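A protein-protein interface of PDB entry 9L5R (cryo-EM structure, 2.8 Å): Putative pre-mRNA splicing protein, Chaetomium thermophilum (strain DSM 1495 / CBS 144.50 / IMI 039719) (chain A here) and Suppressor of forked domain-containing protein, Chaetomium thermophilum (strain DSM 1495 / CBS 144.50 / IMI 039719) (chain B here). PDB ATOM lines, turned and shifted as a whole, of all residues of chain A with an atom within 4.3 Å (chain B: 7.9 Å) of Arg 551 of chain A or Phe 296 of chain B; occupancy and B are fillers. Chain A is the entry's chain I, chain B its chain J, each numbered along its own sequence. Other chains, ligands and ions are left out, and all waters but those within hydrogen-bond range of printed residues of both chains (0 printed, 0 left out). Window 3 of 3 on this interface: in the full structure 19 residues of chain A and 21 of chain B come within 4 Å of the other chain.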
ATOM      1  N   GLU A 516      17.842   7.831  -0.920  1.00  0.00           N
ATOM      2  CA  GLU A 516      18.952   6.884  -0.974  1.00  0.00           C
ATOM      3  C   GLU A 516      19.646   6.919  -2.327  1.00  0.00           C
ATOM      4  O   GLU A 516      20.864   6.740  -2.406  1.00  0.00           O
ATOM      5  CB  GLU A 516      18.471   5.471  -0.668  1.00  0.00           C
ATOM      6  CG  GLU A 516      17.913   5.305   0.715  1.00  0.00           C
ATOM      7  CD  GLU A 516      18.942   4.834   1.703  1.00  0.00           C
ATOM      8  OE1 GLU A 516      20.128   4.753   1.331  1.00  0.00           O
ATOM      9  OE2 GLU A 516      18.567   4.543   2.856  1.00  0.00           O
ATOM     10  N   PHE A 519      21.937   9.882  -2.220  1.00  0.00           N
ATOM     11  CA  PHE A 519      23.107   9.550  -1.415  1.00  0.00           C
ATOM     12  C   PHE A 519      24.063   8.632  -2.160  1.00  0.00           C
ATOM     13  O   PHE A 519      25.282   8.755  -2.007  1.00  0.00           O
ATOM     14  CB  PHE A 519      22.672   8.906  -0.105  1.00  0.00           C
ATOM     15  CG  PHE A 519      22.412   9.887   0.990  1.00  0.00           C
ATOM     16  CD1 PHE A 519      21.423  10.842   0.856  1.00  0.00           C
ATOM     17  CD2 PHE A 519      23.148   9.853   2.156  1.00  0.00           C
ATOM     18  CE1 PHE A 519      21.179  11.747   1.856  1.00  0.00           C
ATOM     19  CE2 PHE A 519      22.908  10.756   3.164  1.00  0.00           C
ATOM     20  CZ  PHE A 519      21.922  11.703   3.013  1.00  0.00           C
ATOM     21  N   LYS A 547      20.095   7.051  12.353  1.00  0.00           N
ATOM     22  CA  LYS A 547      20.888   6.329  11.369  1.00  0.00           C
ATOM     23  C   LYS A 547      21.295   7.215  10.201  1.00  0.00           C
ATOM     24  O   LYS A 547      22.439   7.139   9.741  1.00  0.00           O
ATOM     25  CB  LYS A 547      20.104   5.120  10.864  1.00  0.00           C
ATOM     26  CG  LYS A 547      20.075   3.949  11.832  1.00  0.00           C
ATOM     27  CD  LYS A 547      19.085   2.877  11.419  1.00  0.00           C
ATOM     28  CE  LYS A 547      19.108   2.630   9.929  1.00  0.00           C
ATOM     29  NZ  LYS A 547      18.534   1.309   9.578  1.00  0.00           N
ATOM     30  N   ILE A 548      20.389   8.067   9.724  1.00  0.00           N
ATOM     31  CA  ILE A 548      20.724   8.970   8.625  1.00  0.00           C
ATOM     32  C   ILE A 548      21.738  10.012   9.076  1.00  0.00           C
ATOM     33  O   ILE A 548      22.640  10.397   8.319  1.00  0.00           O
ATOM     34  CB  ILE A 548      19.450   9.615   8.058  1.00  0.00           C
ATOM     35  CG1 ILE A 548      18.537   8.536   7.483  1.00  0.00           C
ATOM     36  CG2 ILE A 548      19.773  10.646   7.012  1.00  0.00           C
ATOM     37  CD1 ILE A 548      19.233   7.511   6.623  1.00  0.00           C
ATOM     38  N   TYR A 549      21.622  10.472  10.321  1.00  0.00           N
ATOM     39  CA  TYR A 549      22.635  11.375  10.853  1.00  0.00           C
ATOM     40  C   TYR A 549      23.998  10.704  10.935  1.00  0.00           C
ATOM     41  O   TYR A 549      25.009  11.331  10.622  1.00  0.00           O
ATOM     42  CB  TYR A 549      22.222  11.897  12.224  1.00  0.00           C
ATOM     43  CG  TYR A 549      21.428  13.173  12.160  1.00  0.00           C
ATOM     44  CD1 TYR A 549      21.963  14.310  11.589  1.00  0.00           C
ATOM     45  CD2 TYR A 549      20.144  13.240  12.670  1.00  0.00           C
ATOM     46  CE1 TYR A 549      21.244  15.475  11.522  1.00  0.00           C
ATOM     47  CE2 TYR A 549      19.420  14.406  12.609  1.00  0.00           C
ATOM     48  CZ  TYR A 549      19.975  15.518  12.033  1.00  0.00           C
ATOM     49  OH  TYR A 549      19.258  16.684  11.967  1.00  0.00           O
ATOM     50  N   GLU A 550      24.041   9.431  11.326  1.00  0.00           N
ATOM     51  CA  GLU A 550      25.306   8.700  11.363  1.00  0.00           C
ATOM     52  C   GLU A 550      25.910   8.542   9.970  1.00  0.00           C
ATOM     53  O   GLU A 550      27.134   8.654   9.791  1.00  0.00           O
ATOM     54  CB  GLU A 550      25.083   7.339  12.005  1.00  0.00           C
ATOM     55  CG  GLU A 550      24.987   7.383  13.502  1.00  0.00           C
ATOM     56  CD  GLU A 550      26.345   7.423  14.149  1.00  0.00           C
ATOM     57  OE1 GLU A 550      27.310   6.933  13.529  1.00  0.00           O
ATOM     58  OE2 GLU A 550      26.456   7.942  15.276  1.00  0.00           O
ATOM     59  N   ARG A 551      25.061   8.278   8.977  1.00  0.00           N
ATOM     60  CA  ARG A 551      25.533   8.161   7.602  1.00  0.00           C
ATOM     61  C   ARG A 551      26.113   9.474   7.093  1.00  0.00           C
ATOM     62  O   ARG A 551      27.189   9.493   6.486  1.00  0.00           O
ATOM     63  CB  ARG A 551      24.393   7.691   6.707  1.00  0.00           C
ATOM     64  CG  ARG A 551      23.956   6.284   7.011  1.00  0.00           C
ATOM     65  CD  ARG A 551      22.796   5.886   6.157  1.00  0.00           C
ATOM     66  NE  ARG A 551      23.162   5.861   4.751  1.00  0.00           N
ATOM     67  CZ  ARG A 551      22.287   5.781   3.762  1.00  0.00           C
ATOM     68  NH1 ARG A 551      20.990   5.710   3.993  1.00  0.00           N
ATOM     69  NH2 ARG A 551      22.725   5.777   2.509  1.00  0.00           N
ATOM     70  N   GLY A 552      25.430  10.585   7.346  1.00  0.00           N
ATOM     71  CA  GLY A 552      25.999  11.873   6.993  1.00  0.00           C
ATOM     72  C   GLY A 552      27.269  12.184   7.757  1.00  0.00           C
ATOM     73  O   GLY A 552      28.172  12.847   7.235  1.00  0.00           O
ATOM     74  N   LEU A 553      27.365  11.692   8.993  1.00  0.00           N
ATOM     75  CA  LEU A 553      28.525  11.977   9.824  1.00  0.00           C
ATOM     76  C   LEU A 553      29.768  11.267   9.319  1.00  0.00           C
ATOM     77  O   LEU A 553      30.875  11.797   9.446  1.00  0.00           O
ATOM     78  CB  LEU A 553      28.251  11.585  11.270  1.00  0.00           C
ATOM     79  CG  LEU A 553      27.569  12.656  12.106  1.00  0.00           C
ATOM     80  CD1 LEU A 553      27.220  12.080  13.441  1.00  0.00           C
ATOM     81  CD2 LEU A 553      28.466  13.843  12.255  1.00  0.00           C
ATOM     82  N   ASP A 554      29.631  10.061   8.780  1.00  0.00           N
ATOM     83  CA  ASP A 554      30.844   9.512   8.184  1.00  0.00           C
ATOM     84  C   ASP A 554      30.989   9.856   6.707  1.00  0.00           C
ATOM     85  O   ASP A 554      32.019   9.529   6.115  1.00  0.00           O
ATOM     86  CB  ASP A 554      30.984   7.993   8.407  1.00  0.00           C
ATOM     87  CG  ASP A 554      30.133   7.141   7.491  1.00  0.00           C
ATOM     88  OD1 ASP A 554      29.157   7.602   6.881  1.00  0.00           O
ATOM     89  OD2 ASP A 554      30.498   5.962   7.348  1.00  0.00           O
ATOM     90  N   LEU A 555      29.994  10.493   6.095  1.00  0.00           N
ATOM     91  CA  LEU A 555      30.213  11.031   4.759  1.00  0.00           C
ATOM     92  C   LEU A 555      30.963  12.357   4.763  1.00  0.00           C
ATOM     93  O   LEU A 555      31.732  12.618   3.834  1.00  0.00           O
ATOM     94  CB  LEU A 555      28.885  11.197   4.026  1.00  0.00           C
ATOM     95  CG  LEU A 555      28.337   9.893   3.461  1.00  0.00           C
ATOM     96  CD1 LEU A 555      27.001  10.120   2.796  1.00  0.00           C
ATOM     97  CD2 LEU A 555      29.326   9.284   2.497  1.00  0.00           C
ATOM     98  N   THR B 258      29.993  -1.990   1.951  1.00  0.00           N
ATOM     99  CA  THR B 258      29.043  -0.959   2.352  1.00  0.00           C
ATOM    100  C   THR B 258      28.846   0.072   1.249  1.00  0.00           C
ATOM    101  O   THR B 258      27.722   0.521   1.005  1.00  0.00           O
ATOM    102  CB  THR B 258      29.529  -0.295   3.634  1.00  0.00           C
ATOM    103  OG1 THR B 258      29.698  -1.294   4.643  1.00  0.00           O
ATOM    104  CG2 THR B 258      28.542   0.719   4.118  1.00  0.00           C
ATOM    105  N   ARG B 259      29.923   0.446   0.560  1.00  0.00           N
ATOM    106  CA  ARG B 259      29.790   1.311  -0.609  1.00  0.00           C
ATOM    107  C   ARG B 259      28.985   0.636  -1.711  1.00  0.00           C
ATOM    108  O   ARG B 259      28.233   1.297  -2.434  1.00  0.00           O
ATOM    109  CB  ARG B 259      31.169   1.706  -1.128  1.00  0.00           C
ATOM    110  CG  ARG B 259      31.706   2.976  -0.523  1.00  0.00           C
ATOM    111  CD  ARG B 259      32.920   3.466  -1.274  1.00  0.00           C
ATOM    112  NE  ARG B 259      34.015   2.506  -1.252  1.00  0.00           N
ATOM    113  CZ  ARG B 259      34.868   2.366  -0.249  1.00  0.00           C
ATOM    114  NH1 ARG B 259      34.773   3.099   0.844  1.00  0.00           N
ATOM    115  NH2 ARG B 259      35.844   1.474  -0.348  1.00  0.00           N
ATOM    116  N   LYS B 261      26.558  -1.322  -1.200  1.00  0.00           N
ATOM    117  CA  LYS B 261      25.257  -1.578  -0.577  1.00  0.00           C
ATOM    118  C   LYS B 261      25.034  -3.046  -0.269  1.00  0.00           C
ATOM    119  O   LYS B 261      23.891  -3.495  -0.185  1.00  0.00           O
ATOM    120  CB  LYS B 261      24.069  -1.045  -1.393  1.00  0.00           C
ATOM    121  CG  LYS B 261      23.965   0.455  -1.503  1.00  0.00           C
ATOM    122  CD  LYS B 261      22.722   0.805  -2.287  1.00  0.00           C
ATOM    123  CE  LYS B 261      22.573   2.293  -2.514  1.00  0.00           C
ATOM    124  NZ  LYS B 261      22.310   3.026  -1.247  1.00  0.00           N
ATOM    125  N   TYR B 263      25.028  -4.806   2.543  1.00  0.00           N
ATOM    126  CA  TYR B 263      25.061  -4.646   3.989  1.00  0.00           C
ATOM    127  C   TYR B 263      25.210  -5.980   4.698  1.00  0.00           C
ATOM    128  O   TYR B 263      25.862  -6.053   5.743  1.00  0.00           O
ATOM    129  CB  TYR B 263      23.811  -3.917   4.454  1.00  0.00           C
ATOM    130  CG  TYR B 263      23.671  -2.563   3.819  1.00  0.00           C
ATOM    131  CD1 TYR B 263      24.754  -1.710   3.736  1.00  0.00           C
ATOM    132  CD2 TYR B 263      22.468  -2.150   3.278  1.00  0.00           C
ATOM    133  CE1 TYR B 263      24.642  -0.484   3.150  1.00  0.00           C
ATOM    134  CE2 TYR B 263      22.347  -0.920   2.691  1.00  0.00           C
ATOM    135  CZ  TYR B 263      23.437  -0.091   2.632  1.00  0.00           C
ATOM    136  OH  TYR B 263      23.325   1.143   2.046  1.00  0.00           O
ATOM    137  N   ALA B 266      28.874  -6.879   4.296  1.00  0.00           N
ATOM    138  CA  ALA B 266      29.661  -6.035   5.187  1.00  0.00           C
ATOM    139  C   ALA B 266      29.545  -6.493   6.633  1.00  0.00           C
ATOM    140  O   ALA B 266      30.546  -6.546   7.357  1.00  0.00           O
ATOM    141  CB  ALA B 266      29.219  -4.584   5.045  1.00  0.00           C
ATOM    142  N   ARG B 267      28.329  -6.840   7.066  1.00  0.00           N
ATOM    143  CA  ARG B 267      28.131  -7.351   8.415  1.00  0.00           C
ATOM    144  C   ARG B 267      28.847  -8.677   8.612  1.00  0.00           C
ATOM    145  O   ARG B 267      29.421  -8.926   9.676  1.00  0.00           O
ATOM    146  CB  ARG B 267      26.639  -7.504   8.689  1.00  0.00           C
ATOM    147  CG  ARG B 267      26.269  -7.599  10.148  1.00  0.00           C
ATOM    148  CD  ARG B 267      24.771  -7.509  10.310  1.00  0.00           C
ATOM    149  NE  ARG B 267      24.311  -6.129  10.250  1.00  0.00           N
ATOM    150  CZ  ARG B 267      23.430  -5.668   9.374  1.00  0.00           C
ATOM    151  NH1 ARG B 267      22.875  -6.457   8.473  1.00  0.00           N
ATOM    152  NH2 ARG B 267      23.100  -4.382   9.404  1.00  0.00           N
ATOM    153  N   TYR B 270      32.627  -7.883   8.984  1.00  0.00           N
ATOM    154  CA  TYR B 270      32.901  -7.313  10.300  1.00  0.00           C
ATOM    155  C   TYR B 270      32.834  -8.380  11.384  1.00  0.00           C
ATOM    156  O   TYR B 270      33.729  -8.478  12.235  1.00  0.00           O
ATOM    157  CB  TYR B 270      31.898  -6.203  10.606  1.00  0.00           C
ATOM    158  CG  TYR B 270      32.189  -4.844  10.016  1.00  0.00           C
ATOM    159  CD1 TYR B 270      33.418  -4.236  10.183  1.00  0.00           C
ATOM    160  CD2 TYR B 270      31.214  -4.156   9.322  1.00  0.00           C
ATOM    161  CE1 TYR B 270      33.673  -2.993   9.654  1.00  0.00           C
ATOM    162  CE2 TYR B 270      31.459  -2.918   8.793  1.00  0.00           C
ATOM    163  CZ  TYR B 270      32.686  -2.337   8.964  1.00  0.00           C
ATOM    164  OH  TYR B 270      32.920  -1.097   8.427  1.00  0.00           O
ATOM    165  N   TYR B 289      32.790  -1.431  13.210  1.00  0.00           N
ATOM    166  CA  TYR B 289      31.556  -2.207  13.260  1.00  0.00           C
ATOM    167  C   TYR B 289      30.467  -1.461  14.013  1.00  0.00           C
ATOM    168  O   TYR B 289      29.294  -1.500  13.624  1.00  0.00           O
ATOM    169  CB  TYR B 289      31.825  -3.556  13.913  1.00  0.00           C
ATOM    170  CG  TYR B 289      30.640  -4.483  13.939  1.00  0.00           C
ATOM    171  CD1 TYR B 289      29.767  -4.557  12.873  1.00  0.00           C
ATOM    172  CD2 TYR B 289      30.398  -5.285  15.032  1.00  0.00           C
ATOM    173  CE1 TYR B 289      28.699  -5.408  12.895  1.00  0.00           C
ATOM    174  CE2 TYR B 289      29.335  -6.134  15.064  1.00  0.00           C
ATOM    175  CZ  TYR B 289      28.487  -6.191  13.997  1.00  0.00           C
ATOM    176  OH  TYR B 289      27.413  -7.041  14.032  1.00  0.00           O
ATOM    177  N   THR B 290      30.839  -0.782  15.099  1.00  0.00           N
ATOM    178  CA  THR B 290      29.875   0.004  15.861  1.00  0.00           C
ATOM    179  C   THR B 290      29.302   1.136  15.026  1.00  0.00           C
ATOM    180  O   THR B 290      28.084   1.350  15.003  1.00  0.00           O
ATOM    181  CB  THR B 290      30.536   0.554  17.116  1.00  0.00           C
ATOM    182  OG1 THR B 290      31.180  -0.515  17.811  1.00  0.00           O
ATOM    183  CG2 THR B 290      29.507   1.179  18.016  1.00  0.00           C
ATOM    184  N   THR B 291      30.168   1.863  14.317  1.00  0.00           N
ATOM    185  CA  THR B 291      29.675   2.930  13.451  1.00  0.00           C
ATOM    186  C   THR B 291      28.827   2.375  12.311  1.00  0.00           C
ATOM    187  O   THR B 291      27.835   2.993  11.906  1.00  0.00           O
ATOM    188  CB  THR B 291      30.839   3.748  12.907  1.00  0.00           C
ATOM    189  OG1 THR B 291      31.776   2.882  12.263  1.00  0.00           O
ATOM    190  CG2 THR B 291      31.531   4.475  14.030  1.00  0.00           C
ATOM    191  N   PHE B 292      29.187   1.193  11.801  1.00  0.00           N
ATOM    192  CA  PHE B 292      28.405   0.562  10.746  1.00  0.00           C
ATOM    193  C   PHE B 292      27.003   0.220  11.218  1.00  0.00           C
ATOM    194  O   PHE B 292      26.028   0.441  10.495  1.00  0.00           O
ATOM    195  CB  PHE B 292      29.102  -0.702  10.259  1.00  0.00           C
ATOM    196  CG  PHE B 292      28.215  -1.596   9.447  1.00  0.00           C
ATOM    197  CD1 PHE B 292      27.840  -1.232   8.171  1.00  0.00           C
ATOM    198  CD2 PHE B 292      27.747  -2.790   9.958  1.00  0.00           C
ATOM    199  CE1 PHE B 292      27.025  -2.036   7.422  1.00  0.00           C
ATOM    200  CE2 PHE B 292      26.926  -3.592   9.210  1.00  0.00           C
ATOM    201  CZ  PHE B 292      26.568  -3.214   7.940  1.00  0.00           C
ATOM    202  N   GLU B 293      26.884  -0.349  12.416  1.00  0.00           N
ATOM    203  CA  GLU B 293      25.564  -0.711  12.910  1.00  0.00           C
ATOM    204  C   GLU B 293      24.749   0.515  13.274  1.00  0.00           C
ATOM    205  O   GLU B 293      23.525   0.507  13.115  1.00  0.00           O
ATOM    206  CB  GLU B 293      25.678  -1.647  14.104  1.00  0.00           C
ATOM    207  CG  GLU B 293      26.310  -2.969  13.775  1.00  0.00           C
ATOM    208  CD  GLU B 293      25.320  -4.013  13.300  1.00  0.00           C
ATOM    209  OE1 GLU B 293      24.270  -3.652  12.741  1.00  0.00           O
ATOM    210  OE2 GLU B 293      25.595  -5.213  13.484  1.00  0.00           O
ATOM    211  N   LYS B 294      25.401   1.576  13.752  1.00  0.00           N
ATOM    212  CA  LYS B 294      24.688   2.829  13.963  1.00  0.00           C
ATOM    213  C   LYS B 294      24.208   3.428  12.653  1.00  0.00           C
ATOM    214  O   LYS B 294      23.223   4.166  12.636  1.00  0.00           O
ATOM    215  CB  LYS B 294      25.577   3.823  14.699  1.00  0.00           C
ATOM    216  CG  LYS B 294      25.806   3.479  16.144  1.00  0.00           C
ATOM    217  CD  LYS B 294      26.394   4.648  16.892  1.00  0.00           C
ATOM    218  CE  LYS B 294      27.872   4.454  17.122  1.00  0.00           C
ATOM    219  NZ  LYS B 294      28.566   5.736  17.378  1.00  0.00           N
ATOM    220  N   GLN B 295      24.893   3.131  11.549  1.00  0.00           N
ATOM    221  CA  GLN B 295      24.476   3.655  10.253  1.00  0.00           C
ATOM    222  C   GLN B 295      23.382   2.819   9.603  1.00  0.00           C
ATOM    223  O   GLN B 295      22.467   3.371   8.985  1.00  0.00           O
ATOM    224  CB  GLN B 295      25.671   3.724   9.316  1.00  0.00           C
ATOM    225  CG  GLN B 295      26.507   4.942   9.464  1.00  0.00           C
ATOM    226  CD  GLN B 295      27.823   4.774   8.788  1.00  0.00           C
ATOM    227  OE1 GLN B 295      27.916   4.875   7.571  1.00  0.00           O
ATOM    228  NE2 GLN B 295      28.858   4.508   9.565  1.00  0.00           N
ATOM    229  N   PHE B 296      23.465   1.493   9.699  1.00  0.00           N
ATOM    230  CA  PHE B 296      22.607   0.618   8.909  1.00  0.00           C
ATOM    231  C   PHE B 296      21.910  -0.481   9.684  1.00  0.00           C
ATOM    232  O   PHE B 296      20.938  -1.038   9.163  1.00  0.00           O
ATOM    233  CB  PHE B 296      23.406  -0.038   7.776  1.00  0.00           C
ATOM    234  CG  PHE B 296      23.992   0.938   6.818  1.00  0.00           C
ATOM    235  CD1 PHE B 296      23.187   1.613   5.927  1.00  0.00           C
ATOM    236  CD2 PHE B 296      25.343   1.199   6.824  1.00  0.00           C
ATOM    237  CE1 PHE B 296      23.722   2.518   5.053  1.00  0.00           C
ATOM    238  CE2 PHE B 296      25.876   2.109   5.957  1.00  0.00           C
ATOM    239  CZ  PHE B 296      25.068   2.767   5.070  1.00  0.00           C
ATOM    240  N   GLY B 297      22.352  -0.822  10.880  1.00  0.00           N
ATOM    241  CA  GLY B 297      21.749  -1.931  11.581  1.00  0.00           C
ATOM    242  C   GLY B 297      20.425  -1.575  12.217  1.00  0.00           C
ATOM    243  O   GLY B 297      20.012  -0.419  12.261  1.00  0.00           O
ATOM    244  N   ASP B 298      19.745  -2.603  12.712  1.00  0.00           N
ATOM    245  CA  ASP B 298      18.531  -2.385  13.478  1.00  0.00           C
ATOM    246  C   ASP B 298      18.883  -1.974  14.903  1.00  0.00           C
ATOM    247  O   ASP B 298      20.044  -2.021  15.322  1.00  0.00           O
ATOM    248  CB  ASP B 298      17.649  -3.633  13.478  1.00  0.00           C
ATOM    249  CG  ASP B 298      18.389  -4.878  13.918  1.00  0.00           C
ATOM    250  OD1 ASP B 298      19.624  -4.824  14.077  1.00  0.00           O
ATOM    251  OD2 ASP B 298      17.731  -5.920  14.107  1.00  0.00           O
ATOM    252  N   LYS B 299      17.853  -1.572  15.651  1.00  0.00           N
ATOM    253  CA  LYS B 299      18.067  -0.979  16.967  1.00  0.00           C
ATOM    254  C   LYS B 299      18.706  -1.967  17.933  1.00  0.00           C
ATOM    255  O   LYS B 299      19.646  -1.616  18.651  1.00  0.00           O
ATOM    256  CB  LYS B 299      16.745  -0.459  17.525  1.00  0.00           C
ATOM    257  CG  LYS B 299      16.896   0.307  18.824  1.00  0.00           C
ATOM    258  CD  LYS B 299      15.666   0.156  19.701  1.00  0.00           C
ATOM    259  CE  LYS B 299      15.788   0.982  20.968  1.00  0.00           C
ATOM    260  NZ  LYS B 299      15.803   2.438  20.675  1.00  0.00           N
ATOM    261  N   VAL B 302      22.175  -2.198  17.344  1.00  0.00           N
ATOM    262  CA  VAL B 302      22.865  -0.991  17.800  1.00  0.00           C
ATOM    263  C   VAL B 302      23.209  -1.088  19.282  1.00  0.00           C
ATOM    264  O   VAL B 302      24.367  -0.893  19.667  1.00  0.00           O
ATOM    265  CB  VAL B 302      22.036   0.267  17.497  1.00  0.00           C
ATOM    266  CG1 VAL B 302      22.671   1.472  18.146  1.00  0.00           C
ATOM    267  CG2 VAL B 302      21.943   0.488  16.014  1.00  0.00           C
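The side-chain carboxylate of Glu 516 of chain A is in salt-bridge range of the side-chain amino group of Lys 261 of chain B, 3.8 Å away. The backbone carbonyl oxygen of Phe 296 of chain B is in hydrogen-bond range of the side-chain amino group of Lys 547 of chain A (3.4 Å). The side-chain carboxylate (OE2) of Glu 550 of chain A is in salt-bridge range of the side-chain amino group (NZ) of Lys 294 of chain B. OE1 of Gln 295 of chain B sits close to OD2 of Asp 554 of chain A (2.8 Å).
Printed residues of chain B within 4 Å of Glu 516 of chain A: Lys 261. Of chain B, only Gln 295 and Phe 296 come within 4 Å of Arg 551 of chain A. Printed residues of chain B within 4 Å of Asp 554 of chain A: Gln 295 (2.8 Å). Of the printed residues of chain A, Lys 294 of chain B touches Lys 547 and Glu 550. Of chain A, only Lys 547 (3.4 Å) and Arg 551 (3.4 Å) come within 4 Å of Phe 296 of chain B. Of the printed residues of chain A, Gly 297 of chain B touches Lys 547. The nearest printed residue of chain B that does not touch Arg 551 of chain A is Lys 261 of chain B (4.7 Å).
OE2 of Glu 516 of chain A lies within salt-bridge range of NH1 of Arg 551 of chain A, 2.9 Å away. The backbone carbonyl oxygen (O) of Thr 291 of chain B sits at hydrogen-bond distance from the side-chain amide nitrogen (NE2) of Gln 295 of chain B.
Lys 294 of chain B touches Lys 547 of chain A (O to CG, 3.3 Å). Lys 547 of chain A touches Gln 295 of chain B (CB to O, 3.5 Å). Lys 547 of chain A touches Gly 297 of chain B (NZ to O, 3.5 Å). Gln 295 of chain B touches Glu 550 of chain A. CG of Gln 295 of chain B touches N of Arg 551 of chain A, 3.7 Å away. Phe 296 of chain B touches Arg 551 of chain A (CE1 to NE, 3.4 Å).
Of the 19 printed residues of chain B, 5 touch a printed residue of chain A. Hydrophobic or aromatic side chains of chain B within 4 Å of the printed part of chain A: Phe 296.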
